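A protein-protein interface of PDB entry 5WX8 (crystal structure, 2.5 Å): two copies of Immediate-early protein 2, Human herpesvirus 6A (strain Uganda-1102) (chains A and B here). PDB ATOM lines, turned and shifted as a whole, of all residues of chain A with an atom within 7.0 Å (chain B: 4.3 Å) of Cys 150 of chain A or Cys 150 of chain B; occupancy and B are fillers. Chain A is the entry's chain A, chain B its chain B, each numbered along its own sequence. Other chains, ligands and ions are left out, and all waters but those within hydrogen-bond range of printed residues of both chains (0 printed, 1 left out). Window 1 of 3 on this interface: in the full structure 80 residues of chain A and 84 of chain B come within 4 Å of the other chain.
Cys 150 of chain A touches three residues of chain B.
Of chain A, only Cys 150 (1.7 Å), Ser 151 (3.3 Å) and Ile 152 (3.6 Å) come within 4 Å of Cys 150 of chain B.
Of the printed residues of chain B, Ile 152 of chain A touches Ile 34 (3.9 Å), Val 149 (3.9 Å) and Cys 150 (3.6 Å).
Of the printed residues of chain B, Val 149 of chain A touches Ile 152 (3.5 Å).
Printed residues of chain A within 4 Å of Ser 151 of chain B: Cys 150 and Ser 151.
Ala 32 of chain B touches none of the printed residues of chain A.
The nearest printed residue of chain B that does not touch Cys 150 of chain A is Ile 34 of chain B (4.6 Å).
The nearest printed residue of chain A that does not touch Ser 151 of chain B is Val 149 of chain A (4.04 Å).
The side-chain sulfur of Cys 150 of chain B forms a disulfide with the side-chain sulfur of Cys 150 of chain A (1.7 Å).
The backbone NH (N) of Ser 151 of chain A lies close to the side-chain sulfur (SG) of Cys 150 of chain B (3.8 Å).
N of Ser 151 of chain A is in hydrogen-bond range of O of Ser 151 of chain B, 3.1 Å away.
The backbone NH (N) of Ile 153 of chain A sits at hydrogen-bond distance from the backbone carbonyl oxygen (O) of Val 149 of chain B (3.0 Å).
O of Asn 30 of chain A is in hydrogen-bond range of N of Ile 152 of chain A, 2.5 Å away.
The backbone NH (N) of Ala 32 of chain A is in hydrogen-bond range of the backbone carbonyl oxygen (O) of Cys 150 of chain A (2.8 Å).
N of Ile 34 of chain A lies within hydrogen-bond range of O of Arg 148 of chain A (2.9 Å).
The backbone NH (N) of Ile 152 of chain B is in hydrogen-bond range of the backbone carbonyl oxygen (O) of Asn 30 of chain B.
The backbone NH (N) of Cys 150 of chain B sits at hydrogen-bond distance from the backbone carbonyl oxygen (O) of Ala 32 of chain B, at 2.6 Å.
Ile 34 of chain A touches Ile 152 of chain B, and with the chains exchanged Ile 152 of chain A touches Ile 34 of chain B.
Val 149 of chain A touches Ile 152 of chain B, and with the chains exchanged Ile 152 of chain A touches Val 149 of chain B.
Cys 150 of chain B touches its own counterpart, Cys 150 of chain A.
Ser 151 of chain A touches its own counterpart, Ser 151 of chain B.
Positions printed for both chains: 22, 30, 31, 32, 34, 149, 150, 151 and 152.
Of the 12 pairs that touch across the chains among the printed residues, 10 have their exchanged pair printed and touching as well.
Among the printed residues, pairs that only touch across the chains: Val 149 of chain A with Ile 152 of chain B, Arg 148 of chain A with Ile 152 of chain B, Cys 150 of chain A with Ser 151 of chain B, Ile 34 of chain A with Ile 152 of chain B, Ile 152 of chain A with Cys 150 of chain B, Cys 150 of chain A with Ile 152 of chain B, Ile 152 of chain A with Val 149 of chain B and Ile 152 of chain A with Ile 34 of chain B.
Printed residues of chain B that touch a printed residue of chain A: Ile 34, Val 149, Cys 150, Ser 151 and Ile 152.
Hydrophobic or aromatic side chains of chain B within 4 Å of the printed part of chain A: Ile 34 and Ile 152.
Printed residues of chain A that touch a printed residue of chain B: Ile 34, Arg 148, Val 149, Cys 150, Ser 151, Ile 152 and Ile 153.
Hydrophobic or aromatic side chains of chain A that line the printed part of chain B: Ile 34, Ile 152 and Ile 153.
Among the printed residues, 12 pairs touch across the chains.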
ATOM      1  N   ILE A  22      14.968  24.565 -13.574  1.00  0.00           N
ATOM      2  CA  ILE A  22      14.852  25.472 -14.716  1.00  0.00           C
ATOM      3  C   ILE A  22      14.710  26.912 -14.236  1.00  0.00           C
ATOM      4  O   ILE A  22      15.378  27.825 -14.736  1.00  0.00           O
ATOM      5  CB  ILE A  22      13.676  25.054 -15.626  1.00  0.00           C
ATOM      6  CG1 ILE A  22      14.068  23.843 -16.476  1.00  0.00           C
ATOM      7  CG2 ILE A  22      13.215  26.220 -16.534  1.00  0.00           C
ATOM      8  CD1 ILE A  22      12.878  23.101 -17.036  1.00  0.00           C
ATOM      9  N   SER A  28      13.891  31.338 -18.009  1.00  0.00           N
ATOM     10  CA  SER A  28      13.152  30.231 -18.594  1.00  0.00           C
ATOM     11  C   SER A  28      13.020  30.372 -20.101  1.00  0.00           C
ATOM     12  O   SER A  28      12.241  29.632 -20.716  1.00  0.00           O
ATOM     13  CB  SER A  28      11.763  30.145 -17.987  1.00  0.00           C
ATOM     14  OG  SER A  28      10.972  31.196 -18.492  1.00  0.00           O
ATOM     15  N   ASN A  30      15.110  29.548 -22.176  1.00  0.00           N
ATOM     16  CA  ASN A  30      15.750  28.432 -22.847  1.00  0.00           C
ATOM     17  C   ASN A  30      15.150  27.105 -22.412  1.00  0.00           C
ATOM     18  O   ASN A  30      15.765  26.059 -22.632  1.00  0.00           O
ATOM     19  CB  ASN A  30      17.259  28.455 -22.609  1.00  0.00           C
ATOM     20  CG  ASN A  30      17.618  28.033 -21.220  1.00  0.00           C
ATOM     21  OD1 ASN A  30      17.029  28.496 -20.235  1.00  0.00           O
ATOM     22  ND2 ASN A  30      18.580  27.130 -21.122  1.00  0.00           N
ATOM     23  N   ALA A  31      13.966  27.121 -21.804  1.00  0.00           N
ATOM     24  CA  ALA A  31      13.279  25.893 -21.425  1.00  0.00           C
ATOM     25  C   ALA A  31      12.158  25.576 -22.404  1.00  0.00           C
ATOM     26  O   ALA A  31      11.780  26.392 -23.259  1.00  0.00           O
ATOM     27  CB  ALA A  31      12.703  25.986 -20.011  1.00  0.00           C
ATOM     28  N   ALA A  32      11.626  24.360 -22.273  1.00  0.00           N
ATOM     29  CA  ALA A  32      10.415  23.999 -23.000  1.00  0.00           C
ATOM     30  C   ALA A  32       9.621  22.971 -22.205  1.00  0.00           C
ATOM     31  O   ALA A  32      10.084  22.420 -21.205  1.00  0.00           O
ATOM     32  CB  ALA A  32      10.724  23.481 -24.414  1.00  0.00           C
ATOM     33  N   ILE A  33       8.390  22.759 -22.648  1.00  0.00           N
ATOM     34  CA  ILE A  33       7.555  21.650 -22.212  1.00  0.00           C
ATOM     35  C   ILE A  33       7.323  20.792 -23.443  1.00  0.00           C
ATOM     36  O   ILE A  33       6.999  21.322 -24.513  1.00  0.00           O
ATOM     37  CB  ILE A  33       6.227  22.153 -21.616  1.00  0.00           C
ATOM     38  CG1 ILE A  33       6.488  23.110 -20.456  1.00  0.00           C
ATOM     39  CG2 ILE A  33       5.384  21.023 -21.139  1.00  0.00           C
ATOM     40  CD1 ILE A  33       5.260  23.916 -20.057  1.00  0.00           C
ATOM     41  N   ILE A  34       7.513  19.482 -23.325  1.00  0.00           N
ATOM     42  CA  ILE A  34       7.142  18.586 -24.417  1.00  0.00           C
ATOM     43  C   ILE A  34       6.092  17.608 -23.923  1.00  0.00           C
ATOM     44  O   ILE A  34       6.229  17.030 -22.837  1.00  0.00           O
ATOM     45  CB  ILE A  34       8.331  17.819 -25.007  1.00  0.00           C
ATOM     46  CG1 ILE A  34       9.573  18.669 -25.029  1.00  0.00           C
ATOM     47  CG2 ILE A  34       7.982  17.379 -26.424  1.00  0.00           C
ATOM     48  CD1 ILE A  34      10.771  17.841 -25.344  1.00  0.00           C
ATOM     49  N   ILE A 118       4.686  21.411 -28.217  1.00  0.00           N
ATOM     50  CA  ILE A 118       5.748  22.103 -27.488  1.00  0.00           C
ATOM     51  C   ILE A 118       5.195  23.385 -26.891  1.00  0.00           C
ATOM     52  O   ILE A 118       4.487  24.142 -27.558  1.00  0.00           O
ATOM     53  CB  ILE A 118       6.962  22.425 -28.372  1.00  0.00           C
ATOM     54  CG1 ILE A 118       7.476  21.161 -29.019  1.00  0.00           C
ATOM     55  CG2 ILE A 118       8.088  22.987 -27.526  1.00  0.00           C
ATOM     56  CD1 ILE A 118       8.327  20.360 -28.096  1.00  0.00           C
ATOM     57  N   PHE A 127       6.370  29.879 -16.585  1.00  0.00           N
ATOM     58  CA  PHE A 127       6.762  28.498 -16.794  1.00  0.00           C
ATOM     59  C   PHE A 127       6.125  27.587 -15.745  1.00  0.00           C
ATOM     60  O   PHE A 127       5.503  26.580 -16.090  1.00  0.00           O
ATOM     61  CB  PHE A 127       8.290  28.400 -16.786  1.00  0.00           C
ATOM     62  CG  PHE A 127       8.799  27.057 -17.183  1.00  0.00           C
ATOM     63  CD1 PHE A 127       9.010  26.749 -18.504  1.00  0.00           C
ATOM     64  CD2 PHE A 127       9.027  26.089 -16.230  1.00  0.00           C
ATOM     65  CE1 PHE A 127       9.453  25.494 -18.872  1.00  0.00           C
ATOM     66  CE2 PHE A 127       9.468  24.838 -16.595  1.00  0.00           C
ATOM     67  CZ  PHE A 127       9.681  24.540 -17.917  1.00  0.00           C
ATOM     68  N   ARG A 148       7.229  16.097 -20.207  1.00  0.00           N
ATOM     69  CA  ARG A 148       8.651  16.240 -19.957  1.00  0.00           C
ATOM     70  C   ARG A 148       9.021  17.704 -20.095  1.00  0.00           C
ATOM     71  O   ARG A 148       8.333  18.474 -20.767  1.00  0.00           O
ATOM     72  CB  ARG A 148       9.479  15.402 -20.939  1.00  0.00           C
ATOM     73  CG  ARG A 148       9.258  13.896 -20.828  1.00  0.00           C
ATOM     74  CD  ARG A 148       9.835  13.394 -19.533  1.00  0.00           C
ATOM     75  NE  ARG A 148       9.937  11.946 -19.469  1.00  0.00           N
ATOM     76  CZ  ARG A 148       9.077  11.179 -18.814  1.00  0.00           C
ATOM     77  NH1 ARG A 148       8.055  11.736 -18.185  1.00  0.00           N
ATOM     78  NH2 ARG A 148       9.235   9.863 -18.791  1.00  0.00           N
ATOM     79  N   VAL A 149      10.131  18.088 -19.477  1.00  0.00           N
ATOM     80  CA  VAL A 149      10.645  19.442 -19.628  1.00  0.00           C
ATOM     81  C   VAL A 149      11.991  19.386 -20.342  1.00  0.00           C
ATOM     82  O   VAL A 149      12.731  18.398 -20.252  1.00  0.00           O
ATOM     83  CB  VAL A 149      10.739  20.161 -18.270  1.00  0.00           C
ATOM     84  CG1 VAL A 149       9.349  20.525 -17.767  1.00  0.00           C
ATOM     85  CG2 VAL A 149      11.437  19.293 -17.279  1.00  0.00           C
ATOM     86  N   CYS A 150      12.297  20.460 -21.068  1.00  0.00           N
ATOM     87  CA  CYS A 150      13.473  20.569 -21.921  1.00  0.00           C
ATOM     88  C   CYS A 150      14.273  21.794 -21.486  1.00  0.00           C
ATOM     89  O   CYS A 150      13.693  22.820 -21.120  1.00  0.00           O
ATOM     90  CB  CYS A 150      13.037  20.680 -23.408  1.00  0.00           C
ATOM     91  SG  CYS A 150      14.217  20.101 -24.740  1.00  0.00           S
ATOM     92  N   SER A 151      15.599  21.677 -21.485  1.00  0.00           N
ATOM     93  CA  SER A 151      16.513  22.816 -21.388  1.00  0.00           C
ATOM     94  C   SER A 151      17.271  22.918 -22.697  1.00  0.00           C
ATOM     95  O   SER A 151      18.019  21.997 -23.052  1.00  0.00           O
ATOM     96  CB  SER A 151      17.509  22.681 -20.235  1.00  0.00           C
ATOM     97  OG  SER A 151      17.030  23.325 -19.068  1.00  0.00           O
ATOM     98  N   ILE A 152      17.085  24.031 -23.402  1.00  0.00           N
ATOM     99  CA  ILE A 152      17.724  24.244 -24.694  1.00  0.00           C
ATOM    100  C   ILE A 152      19.060  24.927 -24.468  1.00  0.00           C
ATOM    101  O   ILE A 152      19.118  26.055 -23.959  1.00  0.00           O
ATOM    102  CB  ILE A 152      16.843  25.065 -25.645  1.00  0.00           C
ATOM    103  CG1 ILE A 152      15.476  24.420 -25.807  1.00  0.00           C
ATOM    104  CG2 ILE A 152      17.495  25.115 -26.997  1.00  0.00           C
ATOM    105  CD1 ILE A 152      14.579  25.156 -26.776  1.00  0.00           C
ATOM    106  N   ILE A 153      20.136  24.247 -24.858  1.00  0.00           N
ATOM    107  CA  ILE A 153      21.475  24.779 -24.647  1.00  0.00           C
ATOM    108  C   ILE A 153      21.651  26.008 -25.534  1.00  0.00           C
ATOM    109  O   ILE A 153      21.550  25.917 -26.764  1.00  0.00           O
ATOM    110  CB  ILE A 153      22.531  23.696 -24.912  1.00  0.00           C
ATOM    111  CG1 ILE A 153      22.058  22.336 -24.355  1.00  0.00           C
ATOM    112  CG2 ILE A 153      23.843  24.070 -24.280  1.00  0.00           C
ATOM    113  CD1 ILE A 153      21.747  22.311 -22.829  1.00  0.00           C
ATOM    114  N   ILE B  22      26.011  15.940 -24.445  1.00  0.00           N
ATOM    115  CA  ILE B  22      24.807  15.118 -24.522  1.00  0.00           C
ATOM    116  C   ILE B  22      25.153  13.646 -24.681  1.00  0.00           C
ATOM    117  O   ILE B  22      24.416  12.775 -24.203  1.00  0.00           O
ATOM    118  CB  ILE B  22      23.897  15.609 -25.652  1.00  0.00           C
ATOM    119  CG1 ILE B  22      23.117  16.816 -25.150  1.00  0.00           C
ATOM    120  CG2 ILE B  22      22.994  14.481 -26.169  1.00  0.00           C
ATOM    121  CD1 ILE B  22      21.946  17.126 -25.998  1.00  0.00           C
ATOM    122  N   ASN B  30      17.377  10.937 -24.420  1.00  0.00           N
ATOM    123  CA  ASN B  30      16.875  12.066 -23.644  1.00  0.00           C
ATOM    124  C   ASN B  30      17.237  13.390 -24.285  1.00  0.00           C
ATOM    125  O   ASN B  30      17.253  14.418 -23.593  1.00  0.00           O
ATOM    126  CB  ASN B  30      17.426  12.042 -22.217  1.00  0.00           C
ATOM    127  CG  ASN B  30      18.924  11.867 -22.189  1.00  0.00           C
ATOM    128  OD1 ASN B  30      19.539  11.632 -23.231  1.00  0.00           O
ATOM    129  ND2 ASN B  30      19.527  11.945 -21.004  1.00  0.00           N
ATOM    130  N   ALA B  31      17.558  13.380 -25.583  1.00  0.00           N
ATOM    131  CA  ALA B  31      18.114  14.538 -26.273  1.00  0.00           C
ATOM    132  C   ALA B  31      17.309  14.848 -27.520  1.00  0.00           C
ATOM    133  O   ALA B  31      16.583  13.998 -28.039  1.00  0.00           O
ATOM    134  CB  ALA B  31      19.569  14.303 -26.674  1.00  0.00           C
ATOM    135  N   ALA B  32      17.466  16.076 -28.010  1.00  0.00           N
ATOM    136  CA  ALA B  32      16.794  16.503 -29.230  1.00  0.00           C
ATOM    137  C   ALA B  32      17.621  17.579 -29.923  1.00  0.00           C
ATOM    138  O   ALA B  32      18.319  18.369 -29.281  1.00  0.00           O
ATOM    139  CB  ALA B  32      15.371  17.044 -28.969  1.00  0.00           C
ATOM    140  N   ILE B  34      16.775  20.778 -32.169  1.00  0.00           N
ATOM    141  CA  ILE B  34      15.695  21.681 -32.541  1.00  0.00           C
ATOM    142  C   ILE B  34      16.233  22.707 -33.521  1.00  0.00           C
ATOM    143  O   ILE B  34      17.333  23.239 -33.333  1.00  0.00           O
ATOM    144  CB  ILE B  34      15.074  22.382 -31.321  1.00  0.00           C
ATOM    145  CG1 ILE B  34      14.667  21.339 -30.286  1.00  0.00           C
ATOM    146  CG2 ILE B  34      13.891  23.213 -31.755  1.00  0.00           C
ATOM    147  CD1 ILE B  34      14.408  21.940 -28.949  1.00  0.00           C
ATOM    148  N   VAL B 149      20.466  22.378 -29.629  1.00  0.00           N
ATOM    149  CA  VAL B 149      20.589  21.058 -29.034  1.00  0.00           C
ATOM    150  C   VAL B 149      19.877  21.088 -27.685  1.00  0.00           C
ATOM    151  O   VAL B 149      20.000  22.072 -26.948  1.00  0.00           O
ATOM    152  CB  VAL B 149      22.080  20.690 -28.918  1.00  0.00           C
ATOM    153  CG1 VAL B 149      22.322  19.740 -27.799  1.00  0.00           C
ATOM    154  CG2 VAL B 149      22.567  20.124 -30.257  1.00  0.00           C
ATOM    155  N   CYS B 150      19.067  20.055 -27.393  1.00  0.00           N
ATOM    156  CA  CYS B 150      18.210  20.046 -26.208  1.00  0.00           C
ATOM    157  C   CYS B 150      18.409  18.787 -25.386  1.00  0.00           C
ATOM    158  O   CYS B 150      18.647  17.701 -25.916  1.00  0.00           O
ATOM    159  CB  CYS B 150      16.681  20.127 -26.544  1.00  0.00           C
ATOM    160  SG  CYS B 150      15.688  20.862 -25.162  1.00  0.00           S
ATOM    161  N   SER B 151      18.227  18.940 -24.083  1.00  0.00           N
ATOM    162  CA  SER B 151      18.264  17.840 -23.135  1.00  0.00           C
ATOM    163  C   SER B 151      16.902  17.738 -22.439  1.00  0.00           C
ATOM    164  O   SER B 151      16.447  18.705 -21.812  1.00  0.00           O
ATOM    165  CB  SER B 151      19.396  18.071 -22.134  1.00  0.00           C
ATOM    166  OG  SER B 151      19.762  16.876 -21.482  1.00  0.00           O
ATOM    167  N   ILE B 152      16.248  16.578 -22.560  1.00  0.00           N
ATOM    168  CA  ILE B 152      14.914  16.352 -22.004  1.00  0.00           C
ATOM    169  C   ILE B 152      15.035  15.533 -20.715  1.00  0.00           C
ATOM    170  O   ILE B 152      15.538  14.399 -20.723  1.00  0.00           O
ATOM    171  CB  ILE B 152      13.997  15.658 -23.019  1.00  0.00           C
ATOM    172  CG1 ILE B 152      13.928  16.469 -24.309  1.00  0.00           C
ATOM    173  CG2 ILE B 152      12.603  15.505 -22.441  1.00  0.00           C
ATOM    174  CD1 ILE B 152      13.592  15.674 -25.531  1.00  0.00           C
